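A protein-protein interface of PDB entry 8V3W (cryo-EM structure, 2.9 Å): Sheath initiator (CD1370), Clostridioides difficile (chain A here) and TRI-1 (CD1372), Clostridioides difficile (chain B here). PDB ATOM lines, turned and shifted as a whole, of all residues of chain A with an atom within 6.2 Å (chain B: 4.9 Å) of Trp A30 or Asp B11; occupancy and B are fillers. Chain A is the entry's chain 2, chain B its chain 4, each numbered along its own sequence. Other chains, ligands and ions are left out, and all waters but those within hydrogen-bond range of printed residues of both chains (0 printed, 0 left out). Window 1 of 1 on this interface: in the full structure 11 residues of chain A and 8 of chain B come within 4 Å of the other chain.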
ATOM      1  N   VAL A  28      18.822 -20.014   1.532  1.00  0.00           N
ATOM      2  CA  VAL A  28      19.748 -20.978   0.956  1.00  0.00           C
ATOM      3  C   VAL A  28      19.129 -21.583  -0.294  1.00  0.00           C
ATOM      4  O   VAL A  28      17.980 -22.040  -0.278  1.00  0.00           O
ATOM      5  CB  VAL A  28      20.099 -22.063   1.983  1.00  0.00           C
ATOM      6  CG1 VAL A  28      21.029 -23.090   1.377  1.00  0.00           C
ATOM      7  CG2 VAL A  28      20.726 -21.440   3.211  1.00  0.00           C
ATOM      8  N   ALA A  29      19.889 -21.594  -1.384  1.00  0.00           N
ATOM      9  CA  ALA A  29      19.374 -22.086  -2.653  1.00  0.00           C
ATOM     10  C   ALA A  29      19.090 -23.582  -2.583  1.00  0.00           C
ATOM     11  O   ALA A  29      19.756 -24.336  -1.871  1.00  0.00           O
ATOM     12  CB  ALA A  29      20.360 -21.797  -3.781  1.00  0.00           C
ATOM     13  N   TRP A  30      18.085 -24.005  -3.345  1.00  0.00           N
ATOM     14  CA  TRP A  30      17.579 -25.369  -3.329  1.00  0.00           C
ATOM     15  C   TRP A  30      17.298 -25.786  -4.762  1.00  0.00           C
ATOM     16  O   TRP A  30      16.854 -24.967  -5.569  1.00  0.00           O
ATOM     17  CB  TRP A  30      16.300 -25.460  -2.479  1.00  0.00           C
ATOM     18  CG  TRP A  30      15.740 -26.836  -2.299  1.00  0.00           C
ATOM     19  CD1 TRP A  30      14.945 -27.515  -3.170  1.00  0.00           C
ATOM     20  CD2 TRP A  30      15.892 -27.681  -1.154  1.00  0.00           C
ATOM     21  NE1 TRP A  30      14.614 -28.741  -2.653  1.00  0.00           N
ATOM     22  CE2 TRP A  30      15.183 -28.866  -1.414  1.00  0.00           C
ATOM     23  CE3 TRP A  30      16.573 -27.555   0.060  1.00  0.00           C
ATOM     24  CZ2 TRP A  30      15.129 -29.915  -0.505  1.00  0.00           C
ATOM     25  CZ3 TRP A  30      16.518 -28.597   0.959  1.00  0.00           C
ATOM     26  CH2 TRP A  30      15.804 -29.764   0.673  1.00  0.00           C
ATOM     27  N   ASP A  31      17.569 -27.045  -5.085  1.00  0.00           N
ATOM     28  CA  ASP A  31      17.280 -27.576  -6.409  1.00  0.00           C
ATOM     29  C   ASP A  31      16.112 -28.549  -6.322  1.00  0.00           C
ATOM     30  O   ASP A  31      16.030 -29.361  -5.397  1.00  0.00           O
ATOM     31  CB  ASP A  31      18.511 -28.245  -7.031  1.00  0.00           C
ATOM     32  CG  ASP A  31      18.792 -29.611  -6.460  1.00  0.00           C
ATOM     33  OD1 ASP A  31      18.697 -29.781  -5.231  1.00  0.00           O
ATOM     34  OD2 ASP A  31      19.120 -30.521  -7.245  1.00  0.00           O
ATOM     35  N   PHE A  32      15.198 -28.450  -7.284  1.00  0.00           N
ATOM     36  CA  PHE A  32      13.899 -29.096  -7.155  1.00  0.00           C
ATOM     37  C   PHE A  32      13.846 -30.492  -7.754  1.00  0.00           C
ATOM     38  O   PHE A  32      13.049 -31.319  -7.297  1.00  0.00           O
ATOM     39  CB  PHE A  32      12.824 -28.217  -7.797  1.00  0.00           C
ATOM     40  CG  PHE A  32      12.825 -26.803  -7.294  1.00  0.00           C
ATOM     41  CD1 PHE A  32      12.455 -26.519  -5.994  1.00  0.00           C
ATOM     42  CD2 PHE A  32      13.198 -25.761  -8.117  1.00  0.00           C
ATOM     43  CE1 PHE A  32      12.449 -25.223  -5.528  1.00  0.00           C
ATOM     44  CE2 PHE A  32      13.195 -24.464  -7.654  1.00  0.00           C
ATOM     45  CZ  PHE A  32      12.821 -24.196  -6.358  1.00  0.00           C
ATOM     46  N   LYS A  34      16.197 -32.724  -7.560  1.00  0.00           N
ATOM     47  CA  LYS A  34      16.906 -33.649  -6.693  1.00  0.00           C
ATOM     48  C   LYS A  34      16.625 -33.435  -5.214  1.00  0.00           C
ATOM     49  O   LYS A  34      17.011 -34.285  -4.404  1.00  0.00           O
ATOM     50  CB  LYS A  34      18.421 -33.554  -6.940  1.00  0.00           C
ATOM     51  CG  LYS A  34      19.132 -34.892  -6.950  1.00  0.00           C
ATOM     52  CD  LYS A  34      20.423 -34.825  -7.751  1.00  0.00           C
ATOM     53  CE  LYS A  34      20.168 -34.331  -9.167  1.00  0.00           C
ATOM     54  NZ  LYS A  34      21.433 -34.145  -9.932  1.00  0.00           N
ATOM     55  N   ASP A  35      15.972 -32.334  -4.841  1.00  0.00           N
ATOM     56  CA  ASP A  35      15.568 -32.064  -3.460  1.00  0.00           C
ATOM     57  C   ASP A  35      16.782 -32.028  -2.529  1.00  0.00           C
ATOM     58  O   ASP A  35      16.913 -32.824  -1.599  1.00  0.00           O
ATOM     59  CB  ASP A  35      14.535 -33.092  -2.987  1.00  0.00           C
ATOM     60  CG  ASP A  35      13.110 -32.621  -3.185  1.00  0.00           C
ATOM     61  OD1 ASP A  35      12.915 -31.457  -3.587  1.00  0.00           O
ATOM     62  OD2 ASP A  35      12.183 -33.419  -2.945  1.00  0.00           O
ATOM     63  N   GLU A  36      17.678 -31.087  -2.805  1.00  0.00           N
ATOM     64  CA  GLU A  36      18.887 -30.893  -2.021  1.00  0.00           C
ATOM     65  C   GLU A  36      19.214 -29.411  -1.938  1.00  0.00           C
ATOM     66  O   GLU A  36      18.805 -28.634  -2.806  1.00  0.00           O
ATOM     67  CB  GLU A  36      20.085 -31.630  -2.640  1.00  0.00           C
ATOM     68  CG  GLU A  36      19.969 -33.135  -2.650  1.00  0.00           C
ATOM     69  CD  GLU A  36      21.111 -33.790  -3.396  1.00  0.00           C
ATOM     70  OE1 GLU A  36      21.901 -33.059  -4.026  1.00  0.00           O
ATOM     71  OE2 GLU A  36      21.221 -35.033  -3.350  1.00  0.00           O
ATOM     72  N   PRO A  37      19.927 -28.989  -0.899  1.00  0.00           N
ATOM     73  CA  PRO A  37      20.596 -27.688  -0.952  1.00  0.00           C
ATOM     74  C   PRO A  37      21.780 -27.744  -1.905  1.00  0.00           C
ATOM     75  O   PRO A  37      22.328 -28.807  -2.199  1.00  0.00           O
ATOM     76  CB  PRO A  37      21.045 -27.449   0.492  1.00  0.00           C
ATOM     77  CG  PRO A  37      21.058 -28.791   1.117  1.00  0.00           C
ATOM     78  CD  PRO A  37      20.002 -29.598   0.437  1.00  0.00           C
ATOM     79  N   ILE A  38      22.171 -26.573  -2.398  1.00  0.00           N
ATOM     80  CA  ILE A  38      23.175 -26.453  -3.449  1.00  0.00           C
ATOM     81  C   ILE A  38      24.472 -25.940  -2.840  1.00  0.00           C
ATOM     82  O   ILE A  38      24.466 -24.967  -2.077  1.00  0.00           O
ATOM     83  CB  ILE A  38      22.689 -25.534  -4.582  1.00  0.00           C
ATOM     84  CG1 ILE A  38      21.886 -26.338  -5.600  1.00  0.00           C
ATOM     85  CG2 ILE A  38      23.856 -24.852  -5.264  1.00  0.00           C
ATOM     86  CD1 ILE A  38      20.929 -25.512  -6.400  1.00  0.00           C
ATOM     87  N   LYS A  45      25.193 -21.925  -1.225  1.00  0.00           N
ATOM     88  CA  LYS A  45      24.946 -20.786  -2.097  1.00  0.00           C
ATOM     89  C   LYS A  45      23.668 -20.080  -1.670  1.00  0.00           C
ATOM     90  O   LYS A  45      22.649 -20.729  -1.420  1.00  0.00           O
ATOM     91  CB  LYS A  45      24.846 -21.240  -3.552  1.00  0.00           C
ATOM     92  CG  LYS A  45      24.162 -20.253  -4.476  1.00  0.00           C
ATOM     93  CD  LYS A  45      23.423 -20.972  -5.586  1.00  0.00           C
ATOM     94  CE  LYS A  45      24.386 -21.499  -6.634  1.00  0.00           C
ATOM     95  NZ  LYS A  45      23.673 -22.005  -7.835  1.00  0.00           N
ATOM     96  N   ILE A  47      20.702 -17.256  -2.467  1.00  0.00           N
ATOM     97  CA  ILE A  47      19.975 -16.460  -3.443  1.00  0.00           C
ATOM     98  C   ILE A  47      19.098 -15.465  -2.689  1.00  0.00           C
ATOM     99  O   ILE A  47      19.005 -15.493  -1.463  1.00  0.00           O
ATOM    100  CB  ILE A  47      19.144 -17.334  -4.397  1.00  0.00           C
ATOM    101  CG1 ILE A  47      18.180 -18.213  -3.604  1.00  0.00           C
ATOM    102  CG2 ILE A  47      20.053 -18.191  -5.257  1.00  0.00           C
ATOM    103  CD1 ILE A  47      17.471 -19.238  -4.441  1.00  0.00           C
ATOM    104  N   VAL A  55      11.681 -20.874  -3.419  1.00  0.00           N
ATOM    105  CA  VAL A  55      12.097 -21.972  -2.547  1.00  0.00           C
ATOM    106  C   VAL A  55      11.147 -22.097  -1.360  1.00  0.00           C
ATOM    107  O   VAL A  55      10.698 -23.197  -1.007  1.00  0.00           O
ATOM    108  CB  VAL A  55      13.550 -21.771  -2.087  1.00  0.00           C
ATOM    109  CG1 VAL A  55      13.909 -22.769  -1.008  1.00  0.00           C
ATOM    110  CG2 VAL A  55      14.492 -21.900  -3.256  1.00  0.00           C
ATOM    111  N   TYR A  58       7.749 -23.535  -2.464  1.00  0.00           N
ATOM    112  CA  TYR A  58       7.841 -24.967  -2.721  1.00  0.00           C
ATOM    113  C   TYR A  58       7.836 -25.749  -1.416  1.00  0.00           C
ATOM    114  O   TYR A  58       7.098 -26.733  -1.265  1.00  0.00           O
ATOM    115  CB  TYR A  58       9.102 -25.251  -3.538  1.00  0.00           C
ATOM    116  CG  TYR A  58       9.377 -26.704  -3.848  1.00  0.00           C
ATOM    117  CD1 TYR A  58      10.068 -27.507  -2.954  1.00  0.00           C
ATOM    118  CD2 TYR A  58       8.972 -27.263  -5.047  1.00  0.00           C
ATOM    119  CE1 TYR A  58      10.331 -28.825  -3.240  1.00  0.00           C
ATOM    120  CE2 TYR A  58       9.230 -28.581  -5.339  1.00  0.00           C
ATOM    121  CZ  TYR A  58       9.911 -29.356  -4.433  1.00  0.00           C
ATOM    122  OH  TYR A  58      10.170 -30.671  -4.723  1.00  0.00           O
ATOM    123  N   LYS A  59       8.631 -25.299  -0.443  1.00  0.00           N
ATOM    124  CA  LYS A  59       8.681 -25.992   0.839  1.00  0.00           C
ATOM    125  C   LYS A  59       7.336 -25.944   1.558  1.00  0.00           C
ATOM    126  O   LYS A  59       6.917 -26.932   2.170  1.00  0.00           O
ATOM    127  CB  LYS A  59       9.783 -25.397   1.712  1.00  0.00           C
ATOM    128  CG  LYS A  59      11.095 -26.143   1.621  1.00  0.00           C
ATOM    129  CD  LYS A  59      12.051 -25.713   2.709  1.00  0.00           C
ATOM    130  CE  LYS A  59      13.214 -24.934   2.135  1.00  0.00           C
ATOM    131  NZ  LYS A  59      14.290 -25.835   1.662  1.00  0.00           N
ATOM    132  N   TYR A  71       6.310 -27.880  13.961  1.00  0.00           N
ATOM    133  CA  TYR A  71       5.628 -26.745  13.359  1.00  0.00           C
ATOM    134  C   TYR A  71       4.430 -26.312  14.200  1.00  0.00           C
ATOM    135  O   TYR A  71       3.964 -27.023  15.091  1.00  0.00           O
ATOM    136  CB  TYR A  71       5.170 -27.082  11.943  1.00  0.00           C
ATOM    137  CG  TYR A  71       6.291 -27.405  10.992  1.00  0.00           C
ATOM    138  CD1 TYR A  71       7.405 -26.587  10.900  1.00  0.00           C
ATOM    139  CD2 TYR A  71       6.233 -28.523  10.182  1.00  0.00           C
ATOM    140  CE1 TYR A  71       8.429 -26.880  10.032  1.00  0.00           C
ATOM    141  CE2 TYR A  71       7.252 -28.823   9.312  1.00  0.00           C
ATOM    142  CZ  TYR A  71       8.347 -27.999   9.241  1.00  0.00           C
ATOM    143  OH  TYR A  71       9.365 -28.298   8.371  1.00  0.00           O
ATOM    144  N   ILE B   4      15.960 -37.023  12.273  1.00  0.00           N
ATOM    145  CA  ILE B   4      15.456 -36.840  10.918  1.00  0.00           C
ATOM    146  C   ILE B   4      13.988 -37.211  10.787  1.00  0.00           C
ATOM    147  O   ILE B   4      13.348 -36.842   9.797  1.00  0.00           O
ATOM    148  CB  ILE B   4      16.301 -37.660   9.923  1.00  0.00           C
ATOM    149  CG1 ILE B   4      16.096 -37.156   8.495  1.00  0.00           C
ATOM    150  CG2 ILE B   4      15.951 -39.130  10.016  1.00  0.00           C
ATOM    151  CD1 ILE B   4      17.105 -36.135   8.059  1.00  0.00           C
ATOM    152  N   LEU B   7      11.209 -34.271  10.467  1.00  0.00           N
ATOM    153  CA  LEU B   7      11.227 -33.339   9.359  1.00  0.00           C
ATOM    154  C   LEU B   7      10.456 -33.894   8.168  1.00  0.00           C
ATOM    155  O   LEU B   7      10.349 -35.114   8.009  1.00  0.00           O
ATOM    156  CB  LEU B   7      12.668 -33.036   8.941  1.00  0.00           C
ATOM    157  CG  LEU B   7      13.436 -32.168   9.933  1.00  0.00           C
ATOM    158  CD1 LEU B   7      14.895 -32.063   9.535  1.00  0.00           C
ATOM    159  CD2 LEU B   7      12.799 -30.800  10.021  1.00  0.00           C
ATOM    160  N   PRO B   8       9.907 -33.029   7.315  1.00  0.00           N
ATOM    161  CA  PRO B   8       9.179 -33.510   6.134  1.00  0.00           C
ATOM    162  C   PRO B   8      10.074 -34.324   5.213  1.00  0.00           C
ATOM    163  O   PRO B   8      11.302 -34.302   5.297  1.00  0.00           O
ATOM    164  CB  PRO B   8       8.692 -32.222   5.462  1.00  0.00           C
ATOM    165  CG  PRO B   8       9.487 -31.128   6.084  1.00  0.00           C
ATOM    166  CD  PRO B   8       9.793 -31.573   7.466  1.00  0.00           C
ATOM    167  N   SER B   9       9.426 -35.047   4.300  1.00  0.00           N
ATOM    168  CA  SER B   9      10.098 -36.102   3.553  1.00  0.00           C
ATOM    169  C   SER B   9      11.086 -35.579   2.519  1.00  0.00           C
ATOM    170  O   SER B   9      11.934 -36.349   2.059  1.00  0.00           O
ATOM    171  CB  SER B   9       9.066 -36.998   2.873  1.00  0.00           C
ATOM    172  OG  SER B   9       8.445 -36.324   1.795  1.00  0.00           O
ATOM    173  N   PHE B  10      11.007 -34.307   2.132  1.00  0.00           N
ATOM    174  CA  PHE B  10      11.991 -33.803   1.183  1.00  0.00           C
ATOM    175  C   PHE B  10      13.354 -33.562   1.817  1.00  0.00           C
ATOM    176  O   PHE B  10      14.318 -33.305   1.090  1.00  0.00           O
ATOM    177  CB  PHE B  10      11.491 -32.520   0.501  1.00  0.00           C
ATOM    178  CG  PHE B  10      11.125 -31.409   1.446  1.00  0.00           C
ATOM    179  CD1 PHE B  10      12.098 -30.690   2.117  1.00  0.00           C
ATOM    180  CD2 PHE B  10       9.802 -31.054   1.627  1.00  0.00           C
ATOM    181  CE1 PHE B  10      11.755 -29.665   2.973  1.00  0.00           C
ATOM    182  CE2 PHE B  10       9.457 -30.027   2.478  1.00  0.00           C
ATOM    183  CZ  PHE B  10      10.433 -29.334   3.151  1.00  0.00           C
ATOM    184  N   ASP B  11      13.458 -33.644   3.140  1.00  0.00           N
ATOM    185  CA  ASP B  11      14.712 -33.448   3.849  1.00  0.00           C
ATOM    186  C   ASP B  11      15.490 -34.743   4.032  1.00  0.00           C
ATOM    187  O   ASP B  11      16.279 -34.851   4.975  1.00  0.00           O
ATOM    188  CB  ASP B  11      14.452 -32.793   5.205  1.00  0.00           C
ATOM    189  CG  ASP B  11      14.370 -31.284   5.113  1.00  0.00           C
ATOM    190  OD1 ASP B  11      15.144 -30.691   4.338  1.00  0.00           O
ATOM    191  OD2 ASP B  11      13.531 -30.688   5.815  1.00  0.00           O
ATOM    192  N   ARG B  12      15.290 -35.722   3.152  1.00  0.00           N
ATOM    193  CA  ARG B  12      15.964 -37.010   3.224  1.00  0.00           C
ATOM    194  C   ARG B  12      17.287 -37.035   2.465  1.00  0.00           C
ATOM    195  O   ARG B  12      17.774 -38.120   2.130  1.00  0.00           O
ATOM    196  CB  ARG B  12      15.046 -38.111   2.693  1.00  0.00           C
ATOM    197  CG  ARG B  12      14.092 -38.692   3.717  1.00  0.00           C
ATOM    198  CD  ARG B  12      14.766 -39.786   4.521  1.00  0.00           C
ATOM    199  NE  ARG B  12      13.816 -40.529   5.338  1.00  0.00           N
ATOM    200  CZ  ARG B  12      13.340 -40.111   6.503  1.00  0.00           C
ATOM    201  NH1 ARG B  12      13.694 -38.945   7.013  1.00  0.00           N
ATOM    202  NH2 ARG B  12      12.485 -40.880   7.169  1.00  0.00           N
ATOM    203  N   ASN B  13      17.870 -35.876   2.171  1.00  0.00           N
ATOM    204  CA  ASN B  13      19.152 -35.841   1.486  1.00  0.00           C
ATOM    205  C   ASN B  13      20.296 -36.068   2.475  1.00  0.00           C
ATOM    206  O   ASN B  13      20.114 -36.062   3.694  1.00  0.00           O
ATOM    207  CB  ASN B  13      19.330 -34.517   0.749  1.00  0.00           C
ATOM    208  CG  ASN B  13      18.932 -33.329   1.588  1.00  0.00           C
ATOM    209  OD1 ASN B  13      17.753 -33.110   1.858  1.00  0.00           O
ATOM    210  ND2 ASN B  13      19.918 -32.548   2.006  1.00  0.00           N
ATOM    211  N   VAL B  16      21.353 -33.025   5.194  1.00  0.00           N
ATOM    212  CA  VAL B  16      20.498 -32.936   6.372  1.00  0.00           C
ATOM    213  C   VAL B  16      20.700 -34.154   7.259  1.00  0.00           C
ATOM    214  O   VAL B  16      20.683 -34.054   8.492  1.00  0.00           O
ATOM    215  CB  VAL B  16      19.025 -32.785   5.948  1.00  0.00           C
ATOM    216  CG1 VAL B  16      18.136 -32.593   7.162  1.00  0.00           C
ATOM    217  CG2 VAL B  16      18.867 -31.639   4.970  1.00  0.00           C
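The indole nitrogen (NE1) of Trp A30 is in hydrogen-bond range of the side-chain carboxylate (OD1) of Asp A35, 3.3 Å away.
The backbone NH (N) of Glu A36 sits at hydrogen-bond distance from the side-chain carboxylate (OD1) of Asp A31.
OD1 of Asp A35 is in hydrogen-bond range of OH of Tyr A58.
Among the printed residues, pairs that only touch across the chains: Pro A37 with Asn B13, Tyr A71 with Pro B8, Asp A35 with Asn B13, Lys A59 with Phe B10, Asp A35 with Phe B10, Glu A36 with Asn B13, Trp A30 with Phe B10 and Trp A30 with Asp B11.
Ile B4 touches none of the printed residues of chain A.
Leu B7 touches none of the printed residues of chain A.
Of the printed residues of chain A, Pro B8 touches Tyr A71.
Asp B11 touches one residue of chain A.
Of the printed residues of chain A, Asn B13 touches Asp A35 (3.6 Å), Glu A36 (3.7 Å) and Pro A37 (3.3 Å).
The nearest residue of chain A that does not touch Asp B11 is Tyr A71 (5.4 Å).
The nearest printed residue of chain B that does not touch Lys A59 is Asp B11 (5.6 Å).
Printed residues of chain A that touch a printed residue of chain B: Trp A30, Asp A35, Glu A36, Pro A37, Lys A59 and Tyr A71.
Hydrophobic or aromatic side chains of chain A within 4 Å of the printed part of chain B: Trp A30, Pro A37 and Tyr A71.
Along chain A the printed residues that touch a printed residue of chain B span positions 30 to 71.
Among the printed residues, 8 pairs touch across the chains.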
